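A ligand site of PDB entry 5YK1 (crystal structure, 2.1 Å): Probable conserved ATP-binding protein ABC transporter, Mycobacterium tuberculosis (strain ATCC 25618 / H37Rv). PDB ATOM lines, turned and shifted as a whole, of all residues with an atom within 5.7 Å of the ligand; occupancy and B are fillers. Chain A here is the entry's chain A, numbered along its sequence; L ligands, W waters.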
ATOM      1  N   ALA A 141       2.459  22.322  30.083  1.00  0.00           N
ATOM      2  CA  ALA A 141       1.041  22.289  29.712  1.00  0.00           C
ATOM      3  C   ALA A 141       0.609  20.942  29.152  1.00  0.00           C
ATOM      4  O   ALA A 141       1.441  20.075  28.889  1.00  0.00           O
ATOM      5  CB  ALA A 141       0.733  23.389  28.695  1.00  0.00           C
ATOM      6  N   SER A 142      -0.693  20.779  28.985  1.00  0.00           N
ATOM      7  CA  SER A 142      -1.223  19.591  28.336  1.00  0.00           C
ATOM      8  C   SER A 142      -1.789  19.954  26.967  1.00  0.00           C
ATOM      9  O   SER A 142      -2.294  21.056  26.755  1.00  0.00           O
ATOM     10  CB  SER A 142      -2.317  18.932  29.185  1.00  0.00           C
ATOM     11  OG  SER A 142      -3.512  19.695  29.130  1.00  0.00           O
ATOM     12  N   ALA A 143      -1.663  19.021  26.032  1.00  0.00           N
ATOM     13  CA  ALA A 143      -2.303  19.111  24.734  1.00  0.00           C
ATOM     14  C   ALA A 143      -3.358  18.016  24.648  1.00  0.00           C
ATOM     15  O   ALA A 143      -3.495  17.223  25.574  1.00  0.00           O
ATOM     16  CB  ALA A 143      -1.278  18.995  23.612  1.00  0.00           C
ATOM     17  N   SER A 144      -4.083  17.954  23.536  1.00  0.00           N
ATOM     18  CA  SER A 144      -5.195  17.009  23.417  1.00  0.00           C
ATOM     19  C   SER A 144      -4.716  15.564  23.480  1.00  0.00           C
ATOM     20  O   SER A 144      -5.310  14.748  24.185  1.00  0.00           O
ATOM     21  CB  SER A 144      -5.977  17.265  22.124  1.00  0.00           C
ATOM     22  OG  SER A 144      -5.120  17.257  20.989  1.00  0.00           O
ATOM     23  N   ILE A 145      -3.639  15.232  22.768  1.00  0.00           N
ATOM     24  CA  ILE A 145      -3.061  13.899  22.883  1.00  0.00           C
ATOM     25  C   ILE A 145      -1.543  13.972  23.110  1.00  0.00           C
ATOM     26  O   ILE A 145      -0.777  13.158  22.596  1.00  0.00           O
ATOM     27  CB  ILE A 145      -3.344  13.024  21.636  1.00  0.00           C
ATOM     28  CG1 ILE A 145      -2.851  13.695  20.350  1.00  0.00           C
ATOM     29  CG2 ILE A 145      -4.836  12.686  21.541  1.00  0.00           C
ATOM     30  CD1 ILE A 145      -2.694  12.722  19.193  1.00  0.00           C
ATOM     31  N   VAL A 148       3.203  19.572  26.683  1.00  0.00           N
ATOM     32  CA  VAL A 148       4.087  20.621  26.220  1.00  0.00           C
ATOM     33  C   VAL A 148       5.133  20.959  27.278  1.00  0.00           C
ATOM     34  O   VAL A 148       4.800  21.227  28.449  1.00  0.00           O
ATOM     35  CB  VAL A 148       3.318  21.900  25.856  1.00  0.00           C
ATOM     36  CG1 VAL A 148       4.271  22.955  25.318  1.00  0.00           C
ATOM     37  CG2 VAL A 148       2.226  21.577  24.841  1.00  0.00           C
ATOM     38  N   ALA A 160       8.704  26.015  22.822  1.00  0.00           N
ATOM     39  CA  ALA A 160       7.734  25.031  23.278  1.00  0.00           C
ATOM     40  C   ALA A 160       7.868  23.762  22.443  1.00  0.00           C
ATOM     41  O   ALA A 160       7.930  23.805  21.198  1.00  0.00           O
ATOM     42  CB  ALA A 160       6.308  25.590  23.189  1.00  0.00           C
ATOM     43  N   LYS A 162       6.003  20.236  21.851  1.00  0.00           N
ATOM     44  CA  LYS A 162       4.834  19.400  22.043  1.00  0.00           C
ATOM     45  C   LYS A 162       5.170  17.953  21.701  1.00  0.00           C
ATOM     46  O   LYS A 162       5.569  17.638  20.563  1.00  0.00           O
ATOM     47  CB  LYS A 162       3.650  19.884  21.203  1.00  0.00           C
ATOM     48  CG  LYS A 162       2.388  19.052  21.427  1.00  0.00           C
ATOM     49  CD  LYS A 162       1.151  19.728  20.890  1.00  0.00           C
ATOM     50  CE  LYS A 162       1.256  20.029  19.411  1.00  0.00           C
ATOM     51  NZ  LYS A 162       0.049  20.740  18.894  1.00  0.00           N
ATOM     52  N   GLU A 209      -4.913  14.952  13.870  1.00  0.00           N
ATOM     53  CA  GLU A 209      -4.527  14.801  15.268  1.00  0.00           C
ATOM     54  C   GLU A 209      -3.188  14.073  15.437  1.00  0.00           C
ATOM     55  O   GLU A 209      -2.394  14.408  16.324  1.00  0.00           O
ATOM     56  CB  GLU A 209      -5.612  14.064  16.064  1.00  0.00           C
ATOM     57  CG  GLU A 209      -6.819  14.935  16.393  1.00  0.00           C
ATOM     58  CD  GLU A 209      -6.490  16.047  17.375  1.00  0.00           C
ATOM     59  OE1 GLU A 209      -5.606  15.851  18.237  1.00  0.00           O
ATOM     60  OE2 GLU A 209      -7.114  17.122  17.286  1.00  0.00           O
ATOM     61  N   TYR A 212       1.729  15.780  13.504  1.00  0.00           N
ATOM     62  CA  TYR A 212       1.983  17.171  13.891  1.00  0.00           C
ATOM     63  C   TYR A 212       2.559  18.025  12.750  1.00  0.00           C
ATOM     64  O   TYR A 212       2.512  19.265  12.786  1.00  0.00           O
ATOM     65  CB  TYR A 212       2.927  17.202  15.088  1.00  0.00           C
ATOM     66  CG  TYR A 212       2.301  16.836  16.429  1.00  0.00           C
ATOM     67  CD1 TYR A 212       0.916  16.780  16.590  1.00  0.00           C
ATOM     68  CD2 TYR A 212       3.094  16.557  17.527  1.00  0.00           C
ATOM     69  CE1 TYR A 212       0.348  16.460  17.827  1.00  0.00           C
ATOM     70  CE2 TYR A 212       2.548  16.236  18.756  1.00  0.00           C
ATOM     71  CZ  TYR A 212       1.186  16.192  18.904  1.00  0.00           C
ATOM     72  OH  TYR A 212       0.666  15.887  20.144  1.00  0.00           O
ATOM     73  N   GLU A 215      -0.167  20.506  10.922  1.00  0.00           N
ATOM     74  CA  GLU A 215      -0.335  21.740  11.671  1.00  0.00           C
ATOM     75  C   GLU A 215       0.912  22.604  11.524  1.00  0.00           C
ATOM     76  O   GLU A 215       0.807  23.820  11.343  1.00  0.00           O
ATOM     77  CB  GLU A 215      -0.623  21.463  13.144  1.00  0.00           C
ATOM     78  CG  GLU A 215      -0.922  22.718  13.938  1.00  0.00           C
ATOM     79  CD  GLU A 215      -0.840  22.501  15.437  1.00  0.00           C
ATOM     80  OE1 GLU A 215      -0.148  21.553  15.864  1.00  0.00           O
ATOM     81  OE2 GLU A 215      -1.465  23.285  16.179  1.00  0.00           O
ATOM     82  N   PRO A 235       4.509  32.496  16.315  1.00  0.00           N
ATOM     83  CA  PRO A 235       5.810  31.890  16.573  1.00  0.00           C
ATOM     84  C   PRO A 235       6.270  31.038  15.404  1.00  0.00           C
ATOM     85  O   PRO A 235       5.456  30.352  14.782  1.00  0.00           O
ATOM     86  CB  PRO A 235       5.568  31.021  17.824  1.00  0.00           C
ATOM     87  CG  PRO A 235       4.091  30.856  17.903  1.00  0.00           C
ATOM     88  CD  PRO A 235       3.481  32.065  17.293  1.00  0.00           C
ATOM     89  N   GLN A 247       8.228  24.936  18.444  1.00  0.00           N
ATOM     90  CA  GLN A 247       8.045  26.302  17.975  1.00  0.00           C
ATOM     91  C   GLN A 247       8.590  27.319  18.971  1.00  0.00           C
ATOM     92  O   GLN A 247       8.799  26.990  20.135  1.00  0.00           O
ATOM     93  CB  GLN A 247       6.569  26.587  17.686  1.00  0.00           C
ATOM     94  CG  GLN A 247       5.681  26.539  18.913  1.00  0.00           C
ATOM     95  CD  GLN A 247       4.201  26.495  18.550  1.00  0.00           C
ATOM     96  OE1 GLN A 247       3.469  27.457  18.792  1.00  0.00           O
ATOM     97  NE2 GLN A 247       3.760  25.380  17.989  1.00  0.00           N
ATOM     98  N   GLU A 248       8.801  28.547  18.515  1.00  0.00           N
ATOM     99  CA  GLU A 248       9.282  29.613  19.389  1.00  0.00           C
ATOM    100  C   GLU A 248       8.335  29.820  20.540  1.00  0.00           C
ATOM    101  O   GLU A 248       7.113  29.769  20.378  1.00  0.00           O
ATOM    102  CB  GLU A 248       9.452  30.904  18.614  1.00  0.00           C
ATOM    103  CG  GLU A 248      10.500  30.837  17.527  1.00  0.00           C
ATOM    104  CD  GLU A 248      10.592  32.133  16.763  1.00  0.00           C
ATOM    105  OE1 GLU A 248       9.535  32.773  16.556  1.00  0.00           O
ATOM    106  OE2 GLU A 248      11.715  32.523  16.385  1.00  0.00           O
ATOM    107  N   TRP A 249       8.896  30.027  21.722  1.00  0.00           N
ATOM    108  CA  TRP A 249       8.103  30.255  22.916  1.00  0.00           C
ATOM    109  C   TRP A 249       7.555  31.678  22.942  1.00  0.00           C
ATOM    110  O   TRP A 249       8.300  32.645  22.818  1.00  0.00           O
ATOM    111  CB  TRP A 249       8.951  30.018  24.183  1.00  0.00           C
ATOM    112  CG  TRP A 249       8.176  30.180  25.450  1.00  0.00           C
ATOM    113  CD1 TRP A 249       7.993  31.337  26.154  1.00  0.00           C
ATOM    114  CD2 TRP A 249       7.456  29.165  26.161  1.00  0.00           C
ATOM    115  NE1 TRP A 249       7.207  31.099  27.261  1.00  0.00           N
ATOM    116  CE2 TRP A 249       6.869  29.770  27.293  1.00  0.00           C
ATOM    117  CE3 TRP A 249       7.259  27.791  25.955  1.00  0.00           C
ATOM    118  CZ2 TRP A 249       6.104  29.062  28.216  1.00  0.00           C
ATOM    119  CZ3 TRP A 249       6.503  27.086  26.879  1.00  0.00           C
ATOM    120  CH2 TRP A 249       5.925  27.722  27.993  1.00  0.00           C
ATOM    121  N   ILE A 250       6.243  31.798  23.080  1.00  0.00           N
ATOM    122  CA  ILE A 250       5.674  33.104  23.339  1.00  0.00           C
ATOM    123  C   ILE A 250       4.728  32.989  24.518  1.00  0.00           C
ATOM    124  O   ILE A 250       4.085  31.961  24.709  1.00  0.00           O
ATOM    125  CB  ILE A 250       4.937  33.705  22.111  1.00  0.00           C
ATOM    126  CG1 ILE A 250       3.730  32.860  21.735  1.00  0.00           C
ATOM    127  CG2 ILE A 250       5.889  33.860  20.917  1.00  0.00           C
ATOM    128  CD1 ILE A 250       2.835  33.526  20.709  1.00  0.00           C
ATOM    129  N   GLU A 251       4.671  34.036  25.325  1.00  0.00           N
ATOM    130  CA  GLU A 251       3.707  34.063  26.408  1.00  0.00           C
ATOM    131  C   GLU A 251       3.178  35.477  26.620  1.00  0.00           C
ATOM    132  O   GLU A 251       3.869  36.465  26.398  1.00  0.00           O
ATOM    133  CB  GLU A 251       4.314  33.512  27.692  1.00  0.00           C
ATOM    134  CG  GLU A 251       5.445  34.349  28.261  1.00  0.00           C
ATOM    135  CD  GLU A 251       5.897  33.844  29.618  1.00  0.00           C
ATOM    136  OE1 GLU A 251       6.196  32.636  29.733  1.00  0.00           O
ATOM    137  OE2 GLU A 251       5.942  34.659  30.563  1.00  0.00           O
ATOM    138  N   GLY A 295      -8.199  29.503  23.783  1.00  0.00           N
ATOM    139  CA  GLY A 295      -6.937  28.838  24.076  1.00  0.00           C
ATOM    140  C   GLY A 295      -5.872  29.086  23.026  1.00  0.00           C
ATOM    141  O   GLY A 295      -4.697  28.950  23.289  1.00  0.00           O
ATOM    142  N   ASN A 296      -6.307  29.482  21.823  1.00  0.00           N
ATOM    143  CA  ASN A 296      -5.379  29.726  20.729  1.00  0.00           C
ATOM    144  C   ASN A 296      -4.726  31.116  20.737  1.00  0.00           C
ATOM    145  O   ASN A 296      -3.822  31.387  19.936  1.00  0.00           O
ATOM    146  CB  ASN A 296      -6.090  29.523  19.384  1.00  0.00           C
ATOM    147  CG  ASN A 296      -6.716  28.139  19.262  1.00  0.00           C
ATOM    148  OD1 ASN A 296      -6.334  27.206  19.956  1.00  0.00           O
ATOM    149  ND2 ASN A 296      -7.691  28.020  18.363  1.00  0.00           N
ATOM    150  N   MET A 298      -3.398  34.972  22.758  1.00  0.00           N
ATOM    151  CA  MET A 298      -2.976  35.695  23.962  1.00  0.00           C
ATOM    152  C   MET A 298      -2.704  37.178  23.677  1.00  0.00           C
ATOM    153  O   MET A 298      -2.513  37.577  22.537  1.00  0.00           O
ATOM    154  CB  MET A 298      -1.727  35.046  24.556  1.00  0.00           C
ATOM    155  CG  MET A 298      -0.519  35.023  23.632  1.00  0.00           C
ATOM    156  SD  MET A 298       0.760  33.883  24.197  1.00  0.00           S
ATOM    157  CE  MET A 298      -0.154  32.346  24.274  1.00  0.00           C
ATOM    158  N   ILE A 308      -1.173  30.796  18.573  1.00  0.00           N
ATOM    159  CA  ILE A 308      -0.306  29.621  18.744  1.00  0.00           C
ATOM    160  C   ILE A 308      -0.807  28.302  18.141  1.00  0.00           C
ATOM    161  O   ILE A 308      -0.010  27.371  17.989  1.00  0.00           O
ATOM    162  CB  ILE A 308      -0.007  29.343  20.228  1.00  0.00           C
ATOM    163  CG1 ILE A 308      -1.300  28.983  20.977  1.00  0.00           C
ATOM    164  CG2 ILE A 308       0.671  30.536  20.869  1.00  0.00           C
ATOM    165  CD1 ILE A 308      -1.059  28.622  22.428  1.00  0.00           C
ATOM    166  N   ASP A 309      -2.090  28.210  17.832  1.00  0.00           N
ATOM    167  CA  ASP A 309      -2.642  26.927  17.358  1.00  0.00           C
ATOM    168  C   ASP A 309      -3.107  27.062  15.908  1.00  0.00           C
ATOM    169  O   ASP A 309      -3.815  27.996  15.561  1.00  0.00           O
ATOM    170  CB  ASP A 309      -3.793  26.477  18.254  1.00  0.00           C
ATOM    171  CG  ASP A 309      -4.210  25.034  18.019  1.00  0.00           C
ATOM    172  OD1 ASP A 309      -3.950  24.478  16.934  1.00  0.00           O
ATOM    173  OD2 ASP A 309      -4.838  24.443  18.923  1.00  0.00           O
ATOM    174  N   PHE A 310      -2.695  26.116  15.066  1.00  0.00           N
ATOM    175  CA  PHE A 310      -3.015  26.189  13.634  1.00  0.00           C
ATOM    176  C   PHE A 310      -3.504  24.855  13.082  1.00  0.00           C
ATOM    177  O   PHE A 310      -3.244  24.511  11.934  1.00  0.00           O
ATOM    178  CB  PHE A 310      -1.785  26.672  12.862  1.00  0.00           C
ATOM    179  CG  PHE A 310      -1.332  28.052  13.263  1.00  0.00           C
ATOM    180  CD1 PHE A 310      -0.419  28.215  14.293  1.00  0.00           C
ATOM    181  CD2 PHE A 310      -1.861  29.173  12.660  1.00  0.00           C
ATOM    182  CE1 PHE A 310      -0.012  29.484  14.683  1.00  0.00           C
ATOM    183  CE2 PHE A 310      -1.470  30.429  13.043  1.00  0.00           C
ATOM    184  CZ  PHE A 310      -0.544  30.588  14.062  1.00  0.00           C
HETATM  185  P1  LIG L   1      -6.041  21.534  20.634  1.00  0.00           P
HETATM  186  O1  LIG L   1      -6.100  21.930  22.163  1.00  0.00           O
HETATM  187  O2  LIG L   1      -6.395  20.002  20.480  1.00  0.00           O
HETATM  188  O3  LIG L   1      -7.049  22.334  19.866  1.00  0.00           O
HETATM  189  P2  LIG L   1      -3.334  21.059  20.962  1.00  0.00           P
HETATM  190  O4  LIG L   1      -3.960  20.614  22.247  1.00  0.00           O
HETATM  191  O5  LIG L   1      -2.771  19.820  20.194  1.00  0.00           O
HETATM  192  N1  LIG L   1      -4.488  21.816  20.012  1.00  0.00           N
HETATM  193  P3  LIG L   1      -2.391  23.606  21.417  1.00  0.00           P
HETATM  194  O6  LIG L   1      -3.829  23.938  21.537  1.00  0.00           O
HETATM  195  O7  LIG L   1      -1.691  24.256  20.208  1.00  0.00           O
HETATM  196  O8  LIG L   1      -2.158  22.032  21.267  1.00  0.00           O
HETATM  197  O9  LIG L   1      -1.697  24.022  22.773  1.00  0.00           O
HETATM  198  C1  LIG L   1      -1.593  23.122  23.887  1.00  0.00           C
HETATM  199  C2  LIG L   1      -0.793  23.799  24.964  1.00  0.00           C
HETATM  200  O10 LIG L   1       0.492  24.182  24.444  1.00  0.00           O
HETATM  201  C3  LIG L   1      -1.433  25.058  25.555  1.00  0.00           C
HETATM  202  O11 LIG L   1      -1.560  24.975  26.970  1.00  0.00           O
HETATM  203  C4  LIG L   1      -0.502  26.202  25.116  1.00  0.00           C
HETATM  204  O12 LIG L   1      -0.364  27.172  26.140  1.00  0.00           O
HETATM  205  C5  LIG L   1       0.820  25.481  24.868  1.00  0.00           C
HETATM  206  N2  LIG L   1       1.642  26.104  23.831  1.00  0.00           N
HETATM  207  C6  LIG L   1       1.648  25.788  22.492  1.00  0.00           C
HETATM  208  N3  LIG L   1       2.462  26.522  21.775  1.00  0.00           N
HETATM  209  C7  LIG L   1       3.040  27.377  22.696  1.00  0.00           C
HETATM  210  C8  LIG L   1       3.992  28.408  22.575  1.00  0.00           C
HETATM  211  N4  LIG L   1       4.566  28.756  21.416  1.00  0.00           N
HETATM  212  N5  LIG L   1       4.342  29.076  23.689  1.00  0.00           N
HETATM  213  C9  LIG L   1       3.774  28.739  24.853  1.00  0.00           C
HETATM  214  N6  LIG L   1       2.861  27.788  25.091  1.00  0.00           N
HETATM  215  C10 LIG L   1       2.539  27.143  23.968  1.00  0.00           C
HETATM  216  O   HOH W   1      -1.925  16.914  20.659  1.00  0.00           O
HETATM  217  O   HOH W   2       1.940  27.996  27.737  1.00  0.00           O
HETATM  218  O   HOH W   3       2.125  30.522  26.916  1.00  0.00           O
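OD1 of Asn 296 lies close to OD2 of Asp 309 (3.3 Å).
OG of Ser 144 sits at hydrogen-bond distance from OE1 of Glu 209 (3.1 Å).
The backbone carbonyl oxygen (O) of Gln 247 sits at hydrogen-bond distance from the backbone NH (N) of Ala 160 (2.9 Å).
The backbone NH of Val 148 sits at hydrogen-bond distance from the backbone carbonyl oxygen of Ala 141, 2.9 Å away.
The side-chain amino group (NZ) of Lys 162 lies within salt-bridge range of the side-chain carboxylate (OE1) of Glu 215, at 3.1 Å.
N of Ile 308 is in hydrogen-bond range of O of Asn 296 (3.0 Å).
The indole nitrogen of Trp 249 lies within hydrogen-bond range of the side-chain carboxylate of Glu 251, at 3.1 Å.
Residues that only touch the ligand: Val 148, Ala 141, Ala 143, Ser 142, Ile 308, Ala 160 and Trp 249.
Hydrophobic or aromatic side chains within 4 Å of the ligand: Ala 141, Ala 143, Val 148, Ala 160, Trp 249 and Ile 308.
13 residues have an atom within 4 Å of the ligand: Ala 141, Ser 142, Ala 143, Ser 144, Val 148, Ala 160, Lys 162, Gln 247, Glu 248, Trp 249, Ile 250, Ile 308 and Asp 309.
The nearest printed residue that does not touch the ligand is Pro 235 (4.1 Å).
N1 of the ligand sits at hydrogen-bond distance from OD2 of Asp 309, 2.9 Å away.
The backbone carbonyl oxygen (O) of Glu 248 is in hydrogen-bond range of a nitrogen (N4) of the ligand (2.9 Å).
The backbone NH (N) of Ser 144 is in hydrogen-bond range of an oxygen (O4) of the ligand, 3.0 Å away.
An oxygen (O2) of the ligand lies within hydrogen-bond range of the side-chain hydroxyl of Ser 144 (3.1 Å).
The backbone NH of Ile 250 is in hydrogen-bond range of a nitrogen (N5) of the ligand (3.4 Å).
A nitrogen (N4) of the ligand lies within hydrogen-bond range of the side-chain amide oxygen (OE1) of Gln 247, at 3.1 Å.
NZ of Lys 162 is in salt-bridge range of O5 of the ligand.
Water W1 lies within hydrogen-bond range of the side-chain hydroxyl (OH) of Tyr 212 (2.8 Å), an oxygen (O5) of the ligand (3.1 Å), the backbone NH (N) of Ile 145 (3.2 Å) and the side-chain hydroxyl (OG) of Ser 144 (3.2 Å).
Water W3 lies within hydrogen-bond range of the backbone carbonyl oxygen (O) of Ile 250 and a nitrogen (N6) of the ligand.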
